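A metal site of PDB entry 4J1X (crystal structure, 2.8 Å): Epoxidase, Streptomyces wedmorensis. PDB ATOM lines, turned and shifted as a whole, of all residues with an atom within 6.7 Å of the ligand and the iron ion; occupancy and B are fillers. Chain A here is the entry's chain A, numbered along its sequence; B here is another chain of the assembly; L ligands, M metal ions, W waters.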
ATOM      1  N   ARG A  96     -18.388  15.740   1.640  1.00  0.00           N
ATOM      2  CA  ARG A  96     -17.559  14.928   2.521  1.00  0.00           C
ATOM      3  C   ARG A  96     -16.943  15.847   3.572  1.00  0.00           C
ATOM      4  O   ARG A  96     -16.139  16.728   3.245  1.00  0.00           O
ATOM      5  CB  ARG A  96     -16.453  14.217   1.734  1.00  0.00           C
ATOM      6  CG  ARG A  96     -16.983  13.181   0.778  1.00  0.00           C
ATOM      7  CD  ARG A  96     -15.882  12.420   0.073  1.00  0.00           C
ATOM      8  NE  ARG A  96     -16.452  11.505  -0.914  1.00  0.00           N
ATOM      9  CZ  ARG A  96     -15.741  10.723  -1.716  1.00  0.00           C
ATOM     10  NH1 ARG A  96     -14.413  10.715  -1.665  1.00  0.00           N
ATOM     11  NH2 ARG A  96     -16.377   9.938  -2.580  1.00  0.00           N
ATOM     12  N   TYR A 102     -17.167  16.943  -4.438  1.00  0.00           N
ATOM     13  CA  TYR A 102     -17.444  16.598  -5.819  1.00  0.00           C
ATOM     14  C   TYR A 102     -18.770  17.176  -6.290  1.00  0.00           C
ATOM     15  O   TYR A 102     -19.559  17.707  -5.504  1.00  0.00           O
ATOM     16  CB  TYR A 102     -17.523  15.073  -5.980  1.00  0.00           C
ATOM     17  CG  TYR A 102     -16.249  14.262  -5.733  1.00  0.00           C
ATOM     18  CD1 TYR A 102     -16.344  12.944  -5.265  1.00  0.00           C
ATOM     19  CD2 TYR A 102     -14.985  14.768  -6.033  1.00  0.00           C
ATOM     20  CE1 TYR A 102     -15.211  12.151  -5.101  1.00  0.00           C
ATOM     21  CE2 TYR A 102     -13.831  13.981  -5.866  1.00  0.00           C
ATOM     22  CZ  TYR A 102     -13.966  12.660  -5.407  1.00  0.00           C
ATOM     23  OH  TYR A 102     -12.848  11.851  -5.241  1.00  0.00           O
ATOM     24  N   TYR A 104     -21.553  15.602  -9.056  1.00  0.00           N
ATOM     25  CA  TYR A 104     -21.847  14.517  -9.981  1.00  0.00           C
ATOM     26  C   TYR A 104     -22.835  14.837 -11.085  1.00  0.00           C
ATOM     27  O   TYR A 104     -23.998  15.119 -10.834  1.00  0.00           O
ATOM     28  CB  TYR A 104     -22.365  13.296  -9.225  1.00  0.00           C
ATOM     29  CG  TYR A 104     -21.420  12.736  -8.210  1.00  0.00           C
ATOM     30  CD1 TYR A 104     -21.442  13.183  -6.894  1.00  0.00           C
ATOM     31  CD2 TYR A 104     -20.526  11.716  -8.557  1.00  0.00           C
ATOM     32  CE1 TYR A 104     -20.608  12.618  -5.937  1.00  0.00           C
ATOM     33  CE2 TYR A 104     -19.694  11.142  -7.597  1.00  0.00           C
ATOM     34  CZ  TYR A 104     -19.745  11.595  -6.290  1.00  0.00           C
ATOM     35  OH  TYR A 104     -18.959  11.000  -5.334  1.00  0.00           O
ATOM     36  N   LEU A 119     -20.448   8.927 -15.143  1.00  0.00           N
ATOM     37  CA  LEU A 119     -20.523  10.266 -14.582  1.00  0.00           C
ATOM     38  C   LEU A 119     -19.449  11.215 -15.075  1.00  0.00           C
ATOM     39  O   LEU A 119     -18.344  10.787 -15.439  1.00  0.00           O
ATOM     40  CB  LEU A 119     -20.347  10.161 -13.065  1.00  0.00           C
ATOM     41  CG  LEU A 119     -21.229   9.211 -12.264  1.00  0.00           C
ATOM     42  CD1 LEU A 119     -20.494   8.822 -10.980  1.00  0.00           C
ATOM     43  CD2 LEU A 119     -22.570   9.893 -11.971  1.00  0.00           C
ATOM     44  N   VAL A 121     -17.448  14.012 -13.444  1.00  0.00           N
ATOM     45  CA  VAL A 121     -17.231  14.498 -12.084  1.00  0.00           C
ATOM     46  C   VAL A 121     -16.396  15.775 -11.978  1.00  0.00           C
ATOM     47  O   VAL A 121     -15.312  15.895 -12.565  1.00  0.00           O
ATOM     48  CB  VAL A 121     -16.564  13.407 -11.208  1.00  0.00           C
ATOM     49  CG1 VAL A 121     -16.419  13.914  -9.776  1.00  0.00           C
ATOM     50  CG2 VAL A 121     -17.399  12.128 -11.248  1.00  0.00           C
ATOM     51  N   VAL A 123     -14.145  17.756  -9.768  1.00  0.00           N
ATOM     52  CA  VAL A 123     -13.277  17.630  -8.600  1.00  0.00           C
ATOM     53  C   VAL A 123     -13.058  19.073  -8.125  1.00  0.00           C
ATOM     54  O   VAL A 123     -12.277  19.841  -8.721  1.00  0.00           O
ATOM     55  CB  VAL A 123     -11.935  16.991  -9.006  1.00  0.00           C
ATOM     56  CG1 VAL A 123     -11.121  16.638  -7.781  1.00  0.00           C
ATOM     57  CG2 VAL A 123     -12.187  15.765  -9.850  1.00  0.00           C
ATOM     58  N   LYS A 132     -10.272  13.192   0.661  1.00  0.00           N
ATOM     59  CA  LYS A 132     -11.177  12.388   1.458  1.00  0.00           C
ATOM     60  C   LYS A 132     -11.584  11.113   0.737  1.00  0.00           C
ATOM     61  O   LYS A 132     -12.151  11.149  -0.360  1.00  0.00           O
ATOM     62  CB  LYS A 132     -12.406  13.210   1.827  1.00  0.00           C
ATOM     63  CG  LYS A 132     -12.006  14.570   2.386  1.00  0.00           C
ATOM     64  CD  LYS A 132     -13.130  15.287   3.101  1.00  0.00           C
ATOM     65  CE  LYS A 132     -12.615  16.578   3.723  1.00  0.00           C
ATOM     66  NZ  LYS A 132     -11.419  16.334   4.588  1.00  0.00           N
ATOM     67  N   ASN A 134     -13.338   7.188   0.176  1.00  0.00           N
ATOM     68  CA  ASN A 134     -14.614   6.531   0.277  1.00  0.00           C
ATOM     69  C   ASN A 134     -14.113   5.173   0.762  1.00  0.00           C
ATOM     70  O   ASN A 134     -12.904   4.915   0.720  1.00  0.00           O
ATOM     71  CB  ASN A 134     -15.301   6.396  -1.092  1.00  0.00           C
ATOM     72  CG  ASN A 134     -14.378   5.861  -2.171  1.00  0.00           C
ATOM     73  OD1 ASN A 134     -13.533   4.994  -1.920  1.00  0.00           O
ATOM     74  ND2 ASN A 134     -14.538   6.363  -3.378  1.00  0.00           N
ATOM     75  N   GLY A 136     -14.167   2.445  -0.599  1.00  0.00           N
ATOM     76  CA  GLY A 136     -14.138   1.532  -1.725  1.00  0.00           C
ATOM     77  C   GLY A 136     -15.597   1.164  -2.011  1.00  0.00           C
ATOM     78  O   GLY A 136     -16.479   1.493  -1.198  1.00  0.00           O
ATOM     79  N   HIS A 137     -15.875   0.495  -3.125  1.00  0.00           N
ATOM     80  CA  HIS A 137     -17.260   0.131  -3.438  1.00  0.00           C
ATOM     81  C   HIS A 137     -17.352  -1.039  -4.415  1.00  0.00           C
ATOM     82  O   HIS A 137     -16.369  -1.403  -5.060  1.00  0.00           O
ATOM     83  CB  HIS A 137     -18.014   1.338  -3.995  1.00  0.00           C
ATOM     84  CG  HIS A 137     -17.318   2.021  -5.126  1.00  0.00           C
ATOM     85  ND1 HIS A 137     -17.097   1.450  -6.371  1.00  0.00           N
ATOM     86  CD2 HIS A 137     -16.758   3.254  -5.191  1.00  0.00           C
ATOM     87  CE1 HIS A 137     -16.441   2.348  -7.132  1.00  0.00           C
ATOM     88  NE2 HIS A 137     -16.203   3.454  -6.456  1.00  0.00           N
ATOM     89  N   GLU A 141     -14.293   0.419 -11.762  1.00  0.00           N
ATOM     90  CA  GLU A 141     -14.494   1.774 -12.216  1.00  0.00           C
ATOM     91  C   GLU A 141     -13.427   2.197 -13.198  1.00  0.00           C
ATOM     92  O   GLU A 141     -12.236   2.065 -12.930  1.00  0.00           O
ATOM     93  CB  GLU A 141     -14.483   2.716 -11.025  1.00  0.00           C
ATOM     94  CG  GLU A 141     -14.901   4.123 -11.333  1.00  0.00           C
ATOM     95  CD  GLU A 141     -14.792   5.009 -10.120  1.00  0.00           C
ATOM     96  OE1 GLU A 141     -14.905   4.469  -8.986  1.00  0.00           O
ATOM     97  OE2 GLU A 141     -14.615   6.236 -10.297  1.00  0.00           O
ATOM     98  N   LEU A 143     -11.758   5.334 -15.296  1.00  0.00           N
ATOM     99  CA  LEU A 143     -11.662   6.790 -15.203  1.00  0.00           C
ATOM    100  C   LEU A 143     -10.827   7.395 -16.317  1.00  0.00           C
ATOM    101  O   LEU A 143      -9.858   6.801 -16.797  1.00  0.00           O
ATOM    102  CB  LEU A 143     -11.102   7.218 -13.849  1.00  0.00           C
ATOM    103  CG  LEU A 143     -11.977   6.866 -12.650  1.00  0.00           C
ATOM    104  CD1 LEU A 143     -11.192   5.960 -11.725  1.00  0.00           C
ATOM    105  CD2 LEU A 143     -12.434   8.132 -11.938  1.00  0.00           C
ATOM    106  N   VAL A 173      -9.815   1.274 -11.324  1.00  0.00           N
ATOM    107  CA  VAL A 173      -9.761   1.006  -9.899  1.00  0.00           C
ATOM    108  C   VAL A 173     -10.648  -0.213  -9.667  1.00  0.00           C
ATOM    109  O   VAL A 173     -11.836  -0.180  -9.976  1.00  0.00           O
ATOM    110  CB  VAL A 173     -10.313   2.192  -9.072  1.00  0.00           C
ATOM    111  CG1 VAL A 173     -10.390   1.825  -7.599  1.00  0.00           C
ATOM    112  CG2 VAL A 173      -9.422   3.402  -9.255  1.00  0.00           C
ATOM    113  N   VAL A 177     -11.558  -1.351  -3.723  1.00  0.00           N
ATOM    114  CA  VAL A 177     -10.357  -0.558  -3.498  1.00  0.00           C
ATOM    115  C   VAL A 177     -10.758   0.877  -3.159  1.00  0.00           C
ATOM    116  O   VAL A 177     -11.511   1.505  -3.891  1.00  0.00           O
ATOM    117  CB  VAL A 177      -9.448  -0.545  -4.754  1.00  0.00           C
ATOM    118  CG1 VAL A 177      -8.230   0.327  -4.498  1.00  0.00           C
ATOM    119  CG2 VAL A 177      -9.033  -1.946  -5.112  1.00  0.00           C
ATOM    120  N   HIS A 179     -10.507   4.925  -2.765  1.00  0.00           N
ATOM    121  CA  HIS A 179      -9.848   5.955  -3.551  1.00  0.00           C
ATOM    122  C   HIS A 179     -10.316   7.365  -3.218  1.00  0.00           C
ATOM    123  O   HIS A 179     -11.320   7.558  -2.549  1.00  0.00           O
ATOM    124  CB  HIS A 179     -10.029   5.674  -5.062  1.00  0.00           C
ATOM    125  CG  HIS A 179     -11.403   5.184  -5.425  1.00  0.00           C
ATOM    126  ND1 HIS A 179     -11.916   3.970  -5.019  1.00  0.00           N
ATOM    127  CD2 HIS A 179     -12.363   5.759  -6.177  1.00  0.00           C
ATOM    128  CE1 HIS A 179     -13.146   3.849  -5.533  1.00  0.00           C
ATOM    129  NE2 HIS A 179     -13.465   4.905  -6.247  1.00  0.00           N
ATOM    130  N   ALA A 180      -9.551   8.343  -3.698  1.00  0.00           N
ATOM    131  CA  ALA A 180      -9.868   9.754  -3.472  1.00  0.00           C
ATOM    132  C   ALA A 180      -9.202  10.580  -4.552  1.00  0.00           C
ATOM    133  O   ALA A 180      -8.136  10.223  -5.049  1.00  0.00           O
ATOM    134  CB  ALA A 180      -9.356  10.178  -2.106  1.00  0.00           C
ATOM    135  N   PHE A 181      -9.834  11.688  -4.914  1.00  0.00           N
ATOM    136  CA  PHE A 181      -9.309  12.568  -5.949  1.00  0.00           C
ATOM    137  C   PHE A 181      -9.410  14.035  -5.528  1.00  0.00           C
ATOM    138  O   PHE A 181     -10.257  14.403  -4.731  1.00  0.00           O
ATOM    139  CB  PHE A 181     -10.120  12.414  -7.244  1.00  0.00           C
ATOM    140  CG  PHE A 181     -10.058  11.045  -7.852  1.00  0.00           C
ATOM    141  CD1 PHE A 181      -8.904  10.602  -8.483  1.00  0.00           C
ATOM    142  CD2 PHE A 181     -11.162  10.189  -7.781  1.00  0.00           C
ATOM    143  CE1 PHE A 181      -8.839   9.320  -9.045  1.00  0.00           C
ATOM    144  CE2 PHE A 181     -11.109   8.913  -8.336  1.00  0.00           C
ATOM    145  CZ  PHE A 181      -9.940   8.474  -8.976  1.00  0.00           C
ATOM    146  N   LEU A 192     -13.101  14.796 -14.373  1.00  0.00           N
ATOM    147  CA  LEU A 192     -12.849  13.477 -14.910  1.00  0.00           C
ATOM    148  C   LEU A 192     -14.142  12.730 -15.184  1.00  0.00           C
ATOM    149  O   LEU A 192     -15.180  13.010 -14.587  1.00  0.00           O
ATOM    150  CB  LEU A 192     -11.932  12.668 -13.965  1.00  0.00           C
ATOM    151  CG  LEU A 192     -12.271  12.566 -12.475  1.00  0.00           C
ATOM    152  CD1 LEU A 192     -13.596  11.882 -12.334  1.00  0.00           C
ATOM    153  CD2 LEU A 192     -11.185  11.801 -11.735  1.00  0.00           C
ATOM    154  N   ALA A 194     -16.094   9.329 -14.944  1.00  0.00           N
ATOM    155  CA  ALA A 194     -16.012   8.115 -14.155  1.00  0.00           C
ATOM    156  C   ALA A 194     -17.074   7.158 -14.625  1.00  0.00           C
ATOM    157  O   ALA A 194     -18.249   7.514 -14.697  1.00  0.00           O
ATOM    158  CB  ALA A 194     -16.216   8.446 -12.678  1.00  0.00           C
ATOM    159  N   ASN A 196     -18.713   3.519 -13.800  1.00  0.00           N
ATOM    160  CA  ASN A 196     -18.848   2.319 -12.959  1.00  0.00           C
ATOM    161  C   ASN A 196     -19.581   1.271 -13.786  1.00  0.00           C
ATOM    162  O   ASN A 196     -20.630   1.562 -14.371  1.00  0.00           O
ATOM    163  CB  ASN A 196     -19.671   2.615 -11.706  1.00  0.00           C
ATOM    164  CG  ASN A 196     -19.016   3.639 -10.814  1.00  0.00           C
ATOM    165  OD1 ASN A 196     -17.997   3.367 -10.156  1.00  0.00           O
ATOM    166  ND2 ASN A 196     -19.578   4.848 -10.792  1.00  0.00           N
ATOM    167  N   GLU B  19     -27.122   5.370  -3.381  1.00  0.00           N
ATOM    168  CA  GLU B  19     -25.794   5.978  -3.408  1.00  0.00           C
ATOM    169  C   GLU B  19     -25.087   5.672  -4.739  1.00  0.00           C
ATOM    170  O   GLU B  19     -24.414   6.520  -5.314  1.00  0.00           O
ATOM    171  CB  GLU B  19     -24.966   5.454  -2.237  1.00  0.00           C
ATOM    172  CG  GLU B  19     -25.557   5.828  -0.891  1.00  0.00           C
ATOM    173  CD  GLU B  19     -24.720   5.342   0.311  1.00  0.00           C
ATOM    174  OE1 GLU B  19     -25.058   5.756   1.453  1.00  0.00           O
ATOM    175  OE2 GLU B  19     -23.752   4.563   0.125  1.00  0.00           O
ATOM    176  N   LYS B  22     -25.820   8.080  -7.275  1.00  0.00           N
ATOM    177  CA  LYS B  22     -25.621   9.404  -6.709  1.00  0.00           C
ATOM    178  C   LYS B  22     -26.895  10.180  -6.432  1.00  0.00           C
ATOM    179  O   LYS B  22     -27.107  11.258  -6.998  1.00  0.00           O
ATOM    180  CB  LYS B  22     -24.706  10.236  -7.623  1.00  0.00           C
ATOM    181  CG  LYS B  22     -23.496   9.492  -8.154  1.00  0.00           C
ATOM    182  CD  LYS B  22     -22.663   8.895  -7.044  1.00  0.00           C
ATOM    183  CE  LYS B  22     -21.496   8.117  -7.629  1.00  0.00           C
ATOM    184  NZ  LYS B  22     -20.888   7.174  -6.635  1.00  0.00           N
HETATM  185  C1  LIG L   1     -15.905   8.441  -7.681  1.00  0.00           C
HETATM  186  C2  LIG L   1     -15.090   9.740  -7.631  1.00  0.00           C
HETATM  187  C3  LIG L   1     -14.493  10.119  -8.983  1.00  0.00           C
HETATM  188  O1  LIG L   1     -16.282   9.019  -4.908  1.00  0.00           O
HETATM  189  O2  LIG L   1     -16.107   6.527  -5.622  1.00  0.00           O
HETATM  190  P1  LIG L   1     -16.667   7.969  -6.031  1.00  0.00           P
HETATM  191  O3  LIG L   1     -15.057   7.390  -8.071  1.00  0.00           O
HETATM  192  O4  LIG L   1     -18.257   7.907  -6.175  1.00  0.00           O
HETATM  193 FE    FE M   1     -15.457   5.355  -7.094  1.00  0.00          FE
HETATM  194  O   HOH W   1     -17.862   5.758  -8.830  1.00  0.00           O
HETATM  195  O   HOH W   2     -13.451   9.113  -3.867  1.00  0.00           O
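O1 of the ligand is in salt-bridge range of NH2 of Arg 96.
ND2 of Asn 134 lies close to O2 of the ligand.
O4 of the ligand lies within salt-bridge range of NZ of Lys 22 of chain B, 2.8 Å away.
The side-chain hydroxyl (OH) of Tyr 104 is in hydrogen-bond range of an oxygen (O4) of the ligand (3.3 Å).
OE1 of Glu 141 lies close to OD1 of Asn 196.
The backbone NH (N) of Val 173 is in hydrogen-bond range of the backbone carbonyl oxygen (O) of Glu 141 (3.0 Å).
OD1 of Asn 134 sits at hydrogen-bond distance from N of His 179.
A ring nitrogen (ND1) of His 179 lies within hydrogen-bond range of the backbone carbonyl oxygen (O) of Val 177, 2.7 Å away.
NH1 of Arg 96 sits at hydrogen-bond distance from O of Lys 132 (2.6 Å).
N of Gly 136 sits at hydrogen-bond distance from OD1 of Asn 134 (2.9 Å).
The side-chain hydroxyl (OH) of Tyr 102 lies within hydrogen-bond range of the backbone NH (N) of Phe 181, at 3.0 Å.
The backbone carbonyl oxygen (O) of Leu 192 lies within hydrogen-bond range of the backbone NH (N) of Val 121, at 2.7 Å.
Residues that only touch the ligand: Tyr 102 (3.3 Å), Phe 181 (3.5 Å) and Leu 192 (3.9 Å).
Hydrophobic or aromatic side chains within 4 Å of the ligand: Tyr 102, Tyr 104, His 137, His 179, Phe 181 and Leu 192.
Asn 134 touches the iron ion.
Of the 22 residues printed, 4 come within 4 Å of the iron ion.
The iron ion is bound by O2 of the ligand (2.0 Å), NE2 of His 137 (2.1 Å), OE1 of Glu 141 (2.2 Å), NE2 of His 179 (2.2 Å) and O3 of the ligand (2.3 Å).
Water W1 lies within hydrogen-bond range of the side-chain amide oxygen of Asn 196 and an oxygen (O4) of the ligand.
Water W2 lies within hydrogen-bond range of the guanidinium group of Arg 96 (2.9 Å), the backbone carbonyl oxygen of His 179 (2.9 Å), the side-chain amide nitrogen of Asn 134 (3.0 Å), an oxygen (O1) of the ligand (3.0 Å) and the side-chain hydroxyl of Tyr 102 (3.1 Å).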
